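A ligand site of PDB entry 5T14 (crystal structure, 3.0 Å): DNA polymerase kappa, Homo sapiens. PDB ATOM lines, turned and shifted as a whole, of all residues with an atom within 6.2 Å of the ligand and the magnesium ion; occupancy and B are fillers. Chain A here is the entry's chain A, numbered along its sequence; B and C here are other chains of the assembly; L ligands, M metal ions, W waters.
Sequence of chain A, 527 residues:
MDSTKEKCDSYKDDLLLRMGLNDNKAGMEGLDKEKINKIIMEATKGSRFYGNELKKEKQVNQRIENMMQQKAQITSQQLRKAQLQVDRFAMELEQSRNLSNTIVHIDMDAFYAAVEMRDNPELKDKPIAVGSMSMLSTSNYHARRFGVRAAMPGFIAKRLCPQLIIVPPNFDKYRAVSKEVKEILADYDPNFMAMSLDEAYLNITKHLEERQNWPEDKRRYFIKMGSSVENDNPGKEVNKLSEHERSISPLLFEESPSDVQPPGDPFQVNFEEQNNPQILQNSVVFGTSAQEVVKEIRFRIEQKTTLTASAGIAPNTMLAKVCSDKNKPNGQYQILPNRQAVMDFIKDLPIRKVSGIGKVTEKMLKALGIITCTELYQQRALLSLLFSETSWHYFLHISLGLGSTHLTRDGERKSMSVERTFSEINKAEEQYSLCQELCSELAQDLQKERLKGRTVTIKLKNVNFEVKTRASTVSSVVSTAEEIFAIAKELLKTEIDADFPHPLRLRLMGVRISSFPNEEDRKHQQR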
ATOM      1  N   ASP A 107     -12.754 -20.798  10.557  1.00  0.00           N
ATOM      2  CA  ASP A 107     -11.902 -21.286   9.472  1.00  0.00           C
ATOM      3  C   ASP A 107     -12.782 -22.121   8.562  1.00  0.00           C
ATOM      4  O   ASP A 107     -13.291 -23.154   8.987  1.00  0.00           O
ATOM      5  CB  ASP A 107     -10.756 -22.124  10.052  1.00  0.00           C
ATOM      6  CG  ASP A 107      -9.695 -22.480   9.028  1.00  0.00           C
ATOM      7  OD1 ASP A 107     -10.014 -22.697   7.838  1.00  0.00           O
ATOM      8  OD2 ASP A 107      -8.506 -22.570   9.424  1.00  0.00           O
ATOM      9  N   MET A 108     -12.954 -21.685   7.313  1.00  0.00           N
ATOM     10  CA  MET A 108     -13.751 -22.464   6.359  1.00  0.00           C
ATOM     11  C   MET A 108     -13.048 -23.777   5.994  1.00  0.00           C
ATOM     12  O   MET A 108     -11.803 -23.865   5.966  1.00  0.00           O
ATOM     13  CB  MET A 108     -14.027 -21.669   5.083  1.00  0.00           C
ATOM     14  CG  MET A 108     -14.825 -20.404   5.306  1.00  0.00           C
ATOM     15  SD  MET A 108     -16.581 -20.715   5.488  1.00  0.00           S
ATOM     16  CE  MET A 108     -16.906 -19.536   6.785  1.00  0.00           C
ATOM     17  N   ASP A 109     -13.883 -24.792   5.722  1.00  0.00           N
ATOM     18  CA  ASP A 109     -13.432 -26.128   5.369  1.00  0.00           C
ATOM     19  C   ASP A 109     -13.212 -26.199   3.872  1.00  0.00           C
ATOM     20  O   ASP A 109     -14.070 -25.765   3.110  1.00  0.00           O
ATOM     21  CB  ASP A 109     -14.474 -27.173   5.768  1.00  0.00           C
ATOM     22  CG  ASP A 109     -14.844 -27.124   7.248  1.00  0.00           C
ATOM     23  OD1 ASP A 109     -13.944 -26.882   8.097  1.00  0.00           O
ATOM     24  OD2 ASP A 109     -16.036 -27.349   7.559  1.00  0.00           O
ATOM     25  N   ALA A 110     -12.080 -26.747   3.467  1.00  0.00           N
ATOM     26  CA  ALA A 110     -11.746 -26.939   2.055  1.00  0.00           C
ATOM     27  C   ALA A 110     -12.259 -25.800   1.152  1.00  0.00           C
ATOM     28  O   ALA A 110     -12.905 -26.052   0.137  1.00  0.00           O
ATOM     29  CB  ALA A 110     -12.291 -28.279   1.587  1.00  0.00           C
ATOM     30  N   PHE A 111     -11.946 -24.564   1.531  1.00  0.00           N
ATOM     31  CA  PHE A 111     -12.719 -23.394   1.075  1.00  0.00           C
ATOM     32  C   PHE A 111     -12.967 -23.304  -0.432  1.00  0.00           C
ATOM     33  O   PHE A 111     -14.109 -23.440  -0.867  1.00  0.00           O
ATOM     34  CB  PHE A 111     -12.112 -22.095   1.622  1.00  0.00           C
ATOM     35  CG  PHE A 111     -12.912 -20.856   1.296  1.00  0.00           C
ATOM     36  CD1 PHE A 111     -14.266 -20.791   1.605  1.00  0.00           C
ATOM     37  CD2 PHE A 111     -12.298 -19.757   0.714  1.00  0.00           C
ATOM     38  CE1 PHE A 111     -14.998 -19.649   1.304  1.00  0.00           C
ATOM     39  CE2 PHE A 111     -13.030 -18.615   0.413  1.00  0.00           C
ATOM     40  CZ  PHE A 111     -14.383 -18.559   0.719  1.00  0.00           C
ATOM     41  N   TYR A 112     -11.911 -23.114  -1.221  1.00  0.00           N
ATOM     42  CA  TYR A 112     -12.108 -22.957  -2.657  1.00  0.00           C
ATOM     43  C   TYR A 112     -12.770 -24.209  -3.235  1.00  0.00           C
ATOM     44  O   TYR A 112     -13.617 -24.105  -4.117  1.00  0.00           O
ATOM     45  CB  TYR A 112     -10.796 -22.643  -3.409  1.00  0.00           C
ATOM     46  CG  TYR A 112     -10.066 -21.340  -3.080  1.00  0.00           C
ATOM     47  CD1 TYR A 112     -10.585 -20.397  -2.188  1.00  0.00           C
ATOM     48  CD2 TYR A 112      -8.861 -21.028  -3.707  1.00  0.00           C
ATOM     49  CE1 TYR A 112      -9.903 -19.225  -1.899  1.00  0.00           C
ATOM     50  CE2 TYR A 112      -8.177 -19.852  -3.428  1.00  0.00           C
ATOM     51  CZ  TYR A 112      -8.700 -18.948  -2.517  1.00  0.00           C
ATOM     52  OH  TYR A 112      -8.015 -17.782  -2.241  1.00  0.00           O
ATOM     53  N   ALA A 113     -12.408 -25.394  -2.719  1.00  0.00           N
ATOM     54  CA  ALA A 113     -12.997 -26.678  -3.146  1.00  0.00           C
ATOM     55  C   ALA A 113     -14.472 -26.823  -2.794  1.00  0.00           C
ATOM     56  O   ALA A 113     -15.277 -27.205  -3.636  1.00  0.00           O
ATOM     57  CB  ALA A 113     -12.212 -27.831  -2.549  1.00  0.00           C
ATOM     58  N   MET A 135      -0.146 -25.852 -10.351  1.00  0.00           N
ATOM     59  CA  MET A 135      -0.253 -25.635  -8.902  1.00  0.00           C
ATOM     60  C   MET A 135      -1.668 -25.806  -8.389  1.00  0.00           C
ATOM     61  O   MET A 135      -2.636 -25.483  -9.080  1.00  0.00           O
ATOM     62  CB  MET A 135       0.253 -24.225  -8.561  1.00  0.00           C
ATOM     63  CG  MET A 135       0.437 -23.930  -7.082  1.00  0.00           C
ATOM     64  SD  MET A 135       1.545 -25.068  -6.227  1.00  0.00           S
ATOM     65  CE  MET A 135       3.070 -24.866  -7.139  1.00  0.00           C
ATOM     66  N   LEU A 136      -1.781 -26.313  -7.156  1.00  0.00           N
ATOM     67  CA  LEU A 136      -3.064 -26.479  -6.484  1.00  0.00           C
ATOM     68  C   LEU A 136      -3.162 -25.588  -5.233  1.00  0.00           C
ATOM     69  O   LEU A 136      -2.369 -25.704  -4.304  1.00  0.00           O
ATOM     70  CB  LEU A 136      -3.262 -27.953  -6.095  1.00  0.00           C
ATOM     71  CG  LEU A 136      -3.142 -29.024  -7.187  1.00  0.00           C
ATOM     72  CD1 LEU A 136      -3.526 -30.375  -6.626  1.00  0.00           C
ATOM     73  CD2 LEU A 136      -4.003 -28.730  -8.410  1.00  0.00           C
ATOM     74  N   SER A 137      -4.137 -24.682  -5.236  1.00  0.00           N
ATOM     75  CA  SER A 137      -4.440 -23.883  -4.063  1.00  0.00           C
ATOM     76  C   SER A 137      -4.882 -24.780  -2.920  1.00  0.00           C
ATOM     77  O   SER A 137      -4.370 -24.670  -1.818  1.00  0.00           O
ATOM     78  CB  SER A 137      -5.560 -22.900  -4.373  1.00  0.00           C
ATOM     79  OG  SER A 137      -5.177 -22.012  -5.415  1.00  0.00           O
ATOM     80  N   THR A 138      -5.855 -25.641  -3.194  1.00  0.00           N
ATOM     81  CA  THR A 138      -6.380 -26.552  -2.199  1.00  0.00           C
ATOM     82  C   THR A 138      -7.034 -27.758  -2.846  1.00  0.00           C
ATOM     83  O   THR A 138      -7.193 -27.810  -4.063  1.00  0.00           O
ATOM     84  CB  THR A 138      -7.413 -25.851  -1.304  1.00  0.00           C
ATOM     85  OG1 THR A 138      -7.736 -26.685  -0.182  1.00  0.00           O
ATOM     86  CG2 THR A 138      -8.699 -25.513  -2.085  1.00  0.00           C
ATOM     87  N   SER A 139      -7.427 -28.691  -1.989  1.00  0.00           N
ATOM     88  CA  SER A 139      -8.170 -29.885  -2.390  1.00  0.00           C
ATOM     89  C   SER A 139      -9.190 -30.234  -1.342  1.00  0.00           C
ATOM     90  O   SER A 139      -9.006 -29.913  -0.161  1.00  0.00           O
ATOM     91  CB  SER A 139      -7.217 -31.040  -2.508  1.00  0.00           C
ATOM     92  OG  SER A 139      -6.639 -31.307  -1.242  1.00  0.00           O
ATOM     93  N   TYR A 141     -11.574 -32.979   0.968  1.00  0.00           N
ATOM     94  CA  TYR A 141     -11.186 -34.068   1.867  1.00  0.00           C
ATOM     95  C   TYR A 141     -11.155 -35.442   1.200  1.00  0.00           C
ATOM     96  O   TYR A 141     -10.309 -36.269   1.549  1.00  0.00           O
ATOM     97  CB  TYR A 141     -12.063 -34.056   3.121  1.00  0.00           C
ATOM     98  CG  TYR A 141     -11.683 -32.924   4.051  1.00  0.00           C
ATOM     99  CD1 TYR A 141     -12.235 -31.656   3.912  1.00  0.00           C
ATOM    100  CD2 TYR A 141     -10.718 -33.103   5.036  1.00  0.00           C
ATOM    101  CE1 TYR A 141     -11.872 -30.615   4.759  1.00  0.00           C
ATOM    102  CE2 TYR A 141     -10.344 -32.072   5.883  1.00  0.00           C
ATOM    103  CZ  TYR A 141     -10.923 -30.836   5.736  1.00  0.00           C
ATOM    104  OH  TYR A 141     -10.546 -29.833   6.573  1.00  0.00           O
ATOM    105  N   ARG A 144      -7.814 -35.549  -0.394  1.00  0.00           N
ATOM    106  CA  ARG A 144      -6.727 -35.576   0.592  1.00  0.00           C
ATOM    107  C   ARG A 144      -6.334 -36.984   1.088  1.00  0.00           C
ATOM    108  O   ARG A 144      -5.176 -37.208   1.459  1.00  0.00           O
ATOM    109  CB  ARG A 144      -7.059 -34.671   1.785  1.00  0.00           C
ATOM    110  CG  ARG A 144      -6.888 -33.212   1.460  1.00  0.00           C
ATOM    111  CD  ARG A 144      -7.167 -32.321   2.651  1.00  0.00           C
ATOM    112  NE  ARG A 144      -7.543 -30.983   2.211  1.00  0.00           N
ATOM    113  CZ  ARG A 144      -7.843 -29.976   3.022  1.00  0.00           C
ATOM    114  NH1 ARG A 144      -7.813 -30.136   4.346  1.00  0.00           N
ATOM    115  NH2 ARG A 144      -8.174 -28.809   2.508  1.00  0.00           N
ATOM    116  N   ALA A 150      -2.756 -28.702  -0.714  1.00  0.00           N
ATOM    117  CA  ALA A 150      -2.343 -27.332  -1.007  1.00  0.00           C
ATOM    118  C   ALA A 150      -0.835 -27.251  -1.287  1.00  0.00           C
ATOM    119  O   ALA A 150      -0.053 -27.889  -0.609  1.00  0.00           O
ATOM    120  CB  ALA A 150      -2.708 -26.421   0.157  1.00  0.00           C
ATOM    121  N   ALA A 151      -0.476 -26.469  -2.308  1.00  0.00           N
ATOM    122  CA  ALA A 151       0.910 -26.218  -2.722  1.00  0.00           C
ATOM    123  C   ALA A 151       1.554 -27.345  -3.528  1.00  0.00           C
ATOM    124  O   ALA A 151       2.712 -27.199  -3.933  1.00  0.00           O
ATOM    125  CB  ALA A 151       1.800 -25.832  -1.547  1.00  0.00           C
ATOM    126  N   SER A 196      -7.764 -13.582   6.374  1.00  0.00           N
ATOM    127  CA  SER A 196      -7.737 -14.072   5.011  1.00  0.00           C
ATOM    128  C   SER A 196      -9.182 -13.989   4.488  1.00  0.00           C
ATOM    129  O   SER A 196     -10.038 -13.371   5.125  1.00  0.00           O
ATOM    130  CB  SER A 196      -7.197 -15.509   5.018  1.00  0.00           C
ATOM    131  OG  SER A 196      -7.828 -16.356   4.072  1.00  0.00           O
ATOM    132  N   ASP A 198     -10.982 -16.895   4.035  1.00  0.00           N
ATOM    133  CA  ASP A 198     -11.638 -18.007   4.733  1.00  0.00           C
ATOM    134  C   ASP A 198     -11.480 -18.017   6.257  1.00  0.00           C
ATOM    135  O   ASP A 198     -12.077 -18.873   6.911  1.00  0.00           O
ATOM    136  CB  ASP A 198     -11.164 -19.357   4.149  1.00  0.00           C
ATOM    137  CG  ASP A 198      -9.991 -19.989   4.912  1.00  0.00           C
ATOM    138  OD1 ASP A 198      -8.956 -19.298   5.051  1.00  0.00           O
ATOM    139  OD2 ASP A 198     -10.096 -21.160   5.351  1.00  0.00           O
ATOM    140  N   GLU A 199     -10.684 -17.109   6.830  1.00  0.00           N
ATOM    141  CA  GLU A 199     -10.367 -17.136   8.270  1.00  0.00           C
ATOM    142  C   GLU A 199     -10.558 -15.798   8.958  1.00  0.00           C
ATOM    143  O   GLU A 199     -10.559 -14.750   8.313  1.00  0.00           O
ATOM    144  CB  GLU A 199      -8.930 -17.634   8.482  1.00  0.00           C
ATOM    145  CG  GLU A 199      -8.816 -19.161   8.386  1.00  0.00           C
ATOM    146  CD  GLU A 199      -7.388 -19.673   8.260  1.00  0.00           C
ATOM    147  OE1 GLU A 199      -6.607 -19.534   9.248  1.00  0.00           O
ATOM    148  OE2 GLU A 199      -7.068 -20.261   7.193  1.00  0.00           O
ATOM    149  N   ASP A 325      -8.338 -26.191  14.318  1.00  0.00           N
ATOM    150  CA  ASP A 325      -7.876 -27.349  13.539  1.00  0.00           C
ATOM    151  C   ASP A 325      -8.327 -28.684  14.154  1.00  0.00           C
ATOM    152  O   ASP A 325      -8.536 -29.659  13.416  1.00  0.00           O
ATOM    153  CB  ASP A 325      -6.348 -27.308  13.415  1.00  0.00           C
ATOM    154  CG  ASP A 325      -5.797 -28.385  12.492  1.00  0.00           C
ATOM    155  OD1 ASP A 325      -6.287 -28.501  11.349  1.00  0.00           O
ATOM    156  OD2 ASP A 325      -4.857 -29.106  12.906  1.00  0.00           O
ATOM    157  N   LYS A 328     -11.823 -30.470  12.759  1.00  0.00           N
ATOM    158  CA  LYS A 328     -12.100 -30.095  11.371  1.00  0.00           C
ATOM    159  C   LYS A 328     -12.271 -31.381  10.561  1.00  0.00           C
ATOM    160  O   LYS A 328     -11.525 -32.329  10.795  1.00  0.00           O
ATOM    161  CB  LYS A 328     -10.930 -29.272  10.826  1.00  0.00           C
ATOM    162  CG  LYS A 328     -11.155 -28.599   9.486  1.00  0.00           C
ATOM    163  CD  LYS A 328      -9.928 -27.792   9.038  1.00  0.00           C
ATOM    164  CE  LYS A 328     -10.077 -26.295   9.301  1.00  0.00           C
ATOM    165  NZ  LYS A 328     -11.012 -25.634   8.349  1.00  0.00           N
ATOM    166  N   PRO A 329     -13.208 -31.464   9.607  1.00  0.00           N
ATOM    167  CA  PRO A 329     -14.120 -30.385   9.213  1.00  0.00           C
ATOM    168  C   PRO A 329     -15.406 -30.354   9.990  1.00  0.00           C
ATOM    169  O   PRO A 329     -15.791 -31.340  10.598  1.00  0.00           O
ATOM    170  CB  PRO A 329     -14.467 -30.729   7.760  1.00  0.00           C
ATOM    171  CG  PRO A 329     -14.094 -32.155   7.583  1.00  0.00           C
ATOM    172  CD  PRO A 329     -12.927 -32.378   8.485  1.00  0.00           C
ATOM    173  P    DT B   4       6.316 -22.388  -8.492  1.00  0.00           P
ATOM    174  OP1  DT B   4       6.947 -21.926  -9.757  1.00  0.00           O
ATOM    175  OP2  DT B   4       6.953 -22.109  -7.183  1.00  0.00           O
ATOM    176  O5'  DT B   4       4.839 -21.809  -8.454  1.00  0.00           O
ATOM    177  C5'  DT B   4       3.988 -21.877  -9.610  1.00  0.00           C
ATOM    178  C4'  DT B   4       2.906 -20.830  -9.501  1.00  0.00           C
ATOM    179  O4'  DT B   4       2.044 -21.150  -8.389  1.00  0.00           O
ATOM    180  C3'  DT B   4       3.421 -19.415  -9.233  1.00  0.00           C
ATOM    181  O3'  DT B   4       2.636 -18.464  -9.960  1.00  0.00           O
ATOM    182  C2'  DT B   4       3.271 -19.263  -7.732  1.00  0.00           C
ATOM    183  C1'  DT B   4       2.053 -20.106  -7.426  1.00  0.00           C
ATOM    184  N1   DT B   4       2.019 -20.723  -6.091  1.00  0.00           N
ATOM    185  C2   DT B   4       0.897 -20.554  -5.318  1.00  0.00           C
ATOM    186  O2   DT B   4      -0.067 -19.898  -5.675  1.00  0.00           O
ATOM    187  N3   DT B   4       0.936 -21.177  -4.098  1.00  0.00           N
ATOM    188  C4   DT B   4       1.974 -21.941  -3.586  1.00  0.00           C
ATOM    189  O4   DT B   4       1.864 -22.449  -2.473  1.00  0.00           O
ATOM    190  C5   DT B   4       3.120 -22.076  -4.450  1.00  0.00           C
ATOM    191  C7   DT B   4       4.287 -22.883  -3.985  1.00  0.00           C
ATOM    192  C6   DT B   4       3.086 -21.482  -5.646  1.00  0.00           C
ATOM    193  O1  VKJ B   5       2.278 -19.299  -1.499  1.00  0.00           O
ATOM    194  C1  VKJ B   5       1.809 -18.263  -1.988  1.00  0.00           C
ATOM    195  N1  VKJ B   5       0.889 -17.577  -1.200  1.00  0.00           N
ATOM    196  C2  VKJ B   5       0.308 -16.394  -1.598  1.00  0.00           C
ATOM    197  N2  VKJ B   5      -0.580 -15.891  -0.726  1.00  0.00           N
ATOM    198  N3  VKJ B   5       0.555 -15.799  -2.763  1.00  0.00           N
ATOM    199  C3  VKJ B   5       1.428 -16.487  -3.532  1.00  0.00           C
ATOM    200  C4  VKJ B   5       2.080 -17.657  -3.241  1.00  0.00           C
ATOM    201  N4  VKJ B   5       2.924 -18.016  -4.270  1.00  0.00           N
ATOM    202  C5  VKJ B   5       2.757 -17.082  -5.167  1.00  0.00           C
ATOM    203  N5  VKJ B   5       1.901 -16.094  -4.744  1.00  0.00           N
ATOM    204  C6  VKJ B   5       1.382 -15.010  -5.548  1.00  0.00           C
ATOM    205  O2  VKJ B   5       0.530 -15.679  -6.499  1.00  0.00           O
ATOM    206  C7  VKJ B   5       2.306 -14.195  -6.438  1.00  0.00           C
ATOM    207  C8  VKJ B   5       1.322 -13.718  -7.494  1.00  0.00           C
ATOM    208  O3  VKJ B   5       0.480 -12.709  -6.938  1.00  0.00           O
ATOM    209  C9  VKJ B   5       0.452 -14.950  -7.734  1.00  0.00           C
ATOM    210  C10 VKJ B   5       0.852 -15.796  -8.920  1.00  0.00           C
ATOM    211  O4  VKJ B   5       2.196 -16.293  -8.744  1.00  0.00           O
ATOM    212  P1  VKJ B   5       3.047 -16.905  -9.963  1.00  0.00           P
ATOM    213  O5  VKJ B   5       4.470 -16.786  -9.602  1.00  0.00           O
ATOM    214  O6  VKJ B   5       2.592 -16.340 -11.251  1.00  0.00           O
ATOM    215  O7  VKJ B   5      -1.640 -12.588   0.348  1.00  0.00           O
ATOM    216  C11 VKJ B   5      -1.329 -13.995   0.470  1.00  0.00           C
ATOM    217  C12 VKJ B   5      -1.285 -14.627  -0.908  1.00  0.00           C
ATOM    218  C13 VKJ B   5      -2.726 -14.810  -1.463  1.00  0.00           C
ATOM    219  C14 VKJ B   5      -2.299 -14.692   1.403  1.00  0.00           C
ATOM    220  O8  VKJ B   5      -2.061 -14.251   2.752  1.00  0.00           O
ATOM    221  C15 VKJ B   5      -3.735 -14.386   0.943  1.00  0.00           C
ATOM    222  O9  VKJ B   5      -4.663 -15.360   1.486  1.00  0.00           O
ATOM    223  C16 VKJ B   5      -3.831 -14.336  -0.550  1.00  0.00           C
ATOM    224  C17 VKJ B   5      -5.102 -14.000  -1.009  1.00  0.00           C
ATOM    225  C18 VKJ B   5      -5.439 -13.915  -2.344  1.00  0.00           C
ATOM    226  C19 VKJ B   5      -4.384 -14.237  -3.313  1.00  0.00           C
ATOM    227  C20 VKJ B   5      -3.007 -14.589  -2.897  1.00  0.00           C
ATOM    228  C21 VKJ B   5      -2.123 -14.912  -3.924  1.00  0.00           C
ATOM    229  C22 VKJ B   5      -2.478 -14.814  -5.270  1.00  0.00           C
ATOM    230  C23 VKJ B   5      -4.737 -14.154  -4.742  1.00  0.00           C
ATOM    231  C24 VKJ B   5      -6.034 -13.789  -5.109  1.00  0.00           C
ATOM    232  C25 VKJ B   5      -7.007 -13.490  -4.137  1.00  0.00           C
ATOM    233  C26 VKJ B   5      -6.719 -13.558  -2.776  1.00  0.00           C
ATOM    234  C27 VKJ B   5      -6.333 -13.712  -6.470  1.00  0.00           C
ATOM    235  C28 VKJ B   5      -3.752 -14.441  -5.684  1.00  0.00           C
ATOM    236  C29 VKJ B   5      -4.063 -14.368  -7.038  1.00  0.00           C
ATOM    237  C30 VKJ B   5      -5.352 -14.002  -7.436  1.00  0.00           C
ATOM    238  P    DC C   9      -2.744 -20.535   7.869  1.00  0.00           P
ATOM    239  OP1  DC C   9      -3.918 -20.468   8.766  1.00  0.00           O
ATOM    240  OP2  DC C   9      -2.140 -21.853   7.487  1.00  0.00           O
ATOM    241  O5'  DC C   9      -3.101 -19.786   6.511  1.00  0.00           O
ATOM    242  C5'  DC C   9      -3.278 -18.347   6.470  1.00  0.00           C
ATOM    243  C4'  DC C   9      -3.970 -17.950   5.188  1.00  0.00           C
ATOM    244  O4'  DC C   9      -2.993 -17.837   4.129  1.00  0.00           O
ATOM    245  C3'  DC C   9      -5.024 -18.936   4.692  1.00  0.00           C
ATOM    246  O3'  DC C   9      -6.130 -18.258   4.096  1.00  0.00           O
ATOM    247  C2'  DC C   9      -4.286 -19.734   3.637  1.00  0.00           C
ATOM    248  C1'  DC C   9      -3.331 -18.715   3.063  1.00  0.00           C
ATOM    249  N1   DC C   9      -2.067 -19.253   2.520  1.00  0.00           N
ATOM    250  C2   DC C   9      -1.559 -18.733   1.321  1.00  0.00           C
ATOM    251  O2   DC C   9      -2.225 -17.865   0.727  1.00  0.00           O
ATOM    252  N3   DC C   9      -0.404 -19.215   0.826  1.00  0.00           N
ATOM    253  C4   DC C   9       0.264 -20.159   1.491  1.00  0.00           C
ATOM    254  N4   DC C   9       1.406 -20.613   0.969  1.00  0.00           N
ATOM    255  C5   DC C   9      -0.220 -20.708   2.719  1.00  0.00           C
ATOM    256  C6   DC C   9      -1.371 -20.219   3.196  1.00  0.00           C
HETATM  257  N1  LIG L   1      -1.354 -21.319  -2.379  1.00  0.00           N
HETATM  258  C1  LIG L   1      -2.471 -20.716  -2.819  1.00  0.00           C
HETATM  259  N2  LIG L   1      -3.682 -20.696  -2.235  1.00  0.00           N
HETATM  260  C2  LIG L   1      -3.686 -21.398  -1.078  1.00  0.00           C
HETATM  261  C3  LIG L   1      -2.612 -22.057  -0.517  1.00  0.00           C
HETATM  262  C4  LIG L   1      -1.393 -22.019  -1.209  1.00  0.00           C
HETATM  263  N3  LIG L   1      -0.280 -22.638  -0.754  1.00  0.00           N
HETATM  264  N4  LIG L   1      -3.002 -22.657   0.674  1.00  0.00           N
HETATM  265  C5  LIG L   1      -4.267 -22.336   0.794  1.00  0.00           C
HETATM  266  N5  LIG L   1      -4.722 -21.570  -0.210  1.00  0.00           N
HETATM  267  P1  LIG L   1      -6.701 -23.101   4.201  1.00  0.00           P
HETATM  268  P2  LIG L   1      -8.613 -25.039   3.175  1.00  0.00           P
HETATM  269  P3  LIG L   1      -8.942 -26.667   5.507  1.00  0.00           P
HETATM  270  C6  LIG L   1      -6.111 -21.071  -0.409  1.00  0.00           C
HETATM  271  O1  LIG L   1      -7.657 -22.799   5.266  1.00  0.00           O
HETATM  272  O2  LIG L   1      -9.587 -24.132   3.767  1.00  0.00           O
HETATM  273  O3  LIG L   1     -10.230 -27.430   5.647  1.00  0.00           O
HETATM  274  C7  LIG L   1      -7.020 -22.219  -0.816  1.00  0.00           C
HETATM  275  O4  LIG L   1      -5.233 -23.233   4.722  1.00  0.00           O
HETATM  276  O5  LIG L   1      -8.864 -25.197   1.586  1.00  0.00           O
HETATM  277  O6  LIG L   1      -7.664 -27.363   5.933  1.00  0.00           O
HETATM  278  C8  LIG L   1      -7.909 -22.456   0.386  1.00  0.00           C
HETATM  279  O7  LIG L   1      -9.256 -22.778  -0.008  1.00  0.00           O
HETATM  280  N6  LIG L   1      -7.107 -24.492   3.464  1.00  0.00           N
HETATM  281  O8  LIG L   1      -8.789 -26.441   3.927  1.00  0.00           O
HETATM  282  O9  LIG L   1      -8.928 -25.281   6.125  1.00  0.00           O
HETATM  283  C9  LIG L   1      -7.862 -21.138   1.152  1.00  0.00           C
HETATM  284  O10 LIG L   1      -6.616 -20.522   0.803  1.00  0.00           O
HETATM  285  C10 LIG L   1      -7.930 -21.325   2.648  1.00  0.00           C
HETATM  286  O11 LIG L   1      -6.723 -21.932   3.100  1.00  0.00           O
HETATM  287 MG    MG M   1      -9.707 -23.276   5.770  1.00  0.00          MG
HETATM  288  O   HOH W   1      -0.313 -23.982   2.093  1.00  0.00           O
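The side-chain hydroxyl of Thr 138 lies within hydrogen-bond range of an oxygen (O5) of the ligand, 2.6 Å away. An oxygen (O3) of the ligand lies within salt-bridge range of the side-chain amino group of Lys 328. The backbone NH of Phe 111 sits at hydrogen-bond distance from an oxygen (O5) of the ligand, 3.1 Å away. A nitrogen (N3) of the ligand is in hydrogen-bond range of N4 of DC 9 of chain C (3.1 Å). A nitrogen (N3) of the ligand sits at hydrogen-bond distance from O4 of DT 4 of chain B (2.8 Å). The backbone NH of Tyr 112 sits at hydrogen-bond distance from an oxygen (O7) of the ligand, 2.9 Å away. The backbone NH of Ala 110 lies within hydrogen-bond range of an oxygen (O3) of the ligand, 2.9 Å away. O6 of the ligand lies within salt-bridge range of NH1 of Arg 144 (3.2 Å). The side-chain hydroxyl (OH) of Tyr 141 sits at hydrogen-bond distance from an oxygen (O3) of the ligand, at 2.6 Å.
NZ of Lys 328 sits close to O of Met 108, 3.1 Å away. The side-chain hydroxyl of Ser 196 lies within hydrogen-bond range of the backbone NH of Asp 198, at 3.2 Å. O of Ser 139 is in hydrogen-bond range of NE of Arg 144 (3.0 Å). The backbone carbonyl oxygen (O) of Asp 107 sits at hydrogen-bond distance from the side-chain amino group (NZ) of Lys 328 (3.4 Å). O3' of DC 9 of chain C is in hydrogen-bond range of the side-chain hydroxyl (OG) of Ser 196 (2.5 Å). N of Ala 151 is in hydrogen-bond range of O of Leu 136. The guanidinium group (NH2) of Arg 144 is in hydrogen-bond range of the side-chain hydroxyl (OG1) of Thr 138 (3.5 Å). N3 of DC 9 of chain C sits at hydrogen-bond distance from N1 of VKJ 5 of chain B (2.9 Å).
A nitrogen (N4) of the ligand sits close to the backbone carbonyl oxygen of Ser 137 (3.5 Å). An oxygen (O1) of the ligand lies close to the side-chain carboxylate of Glu 199, 3.2 Å away. Asp 109 touches the ligand. CB of Ala 150 touches N4 of the ligand, 3.8 Å away. Ala 151 touches the ligand. Hydrophobic or aromatic side chains within 4 Å of the ligand: Phe 111, Tyr 112, Tyr 141, Ala 150 and Ala 151. Of the 25 residues printed, 17 come within 4 Å of the ligand.
NZ of Lys 328 touches the magnesium ion, 3.7 Å away. Of the 25 residues printed, 4 come within 4 Å of the magnesium ion.
The magnesium ion is bound by O1 of the ligand (2.2 Å), OD1 of Asp 107 (2.2 Å), O9 of the ligand (2.2 Å), O2 of the ligand (2.2 Å), O of Met 108 (2.2 Å) and OD2 of Asp 198 (2.2 Å).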
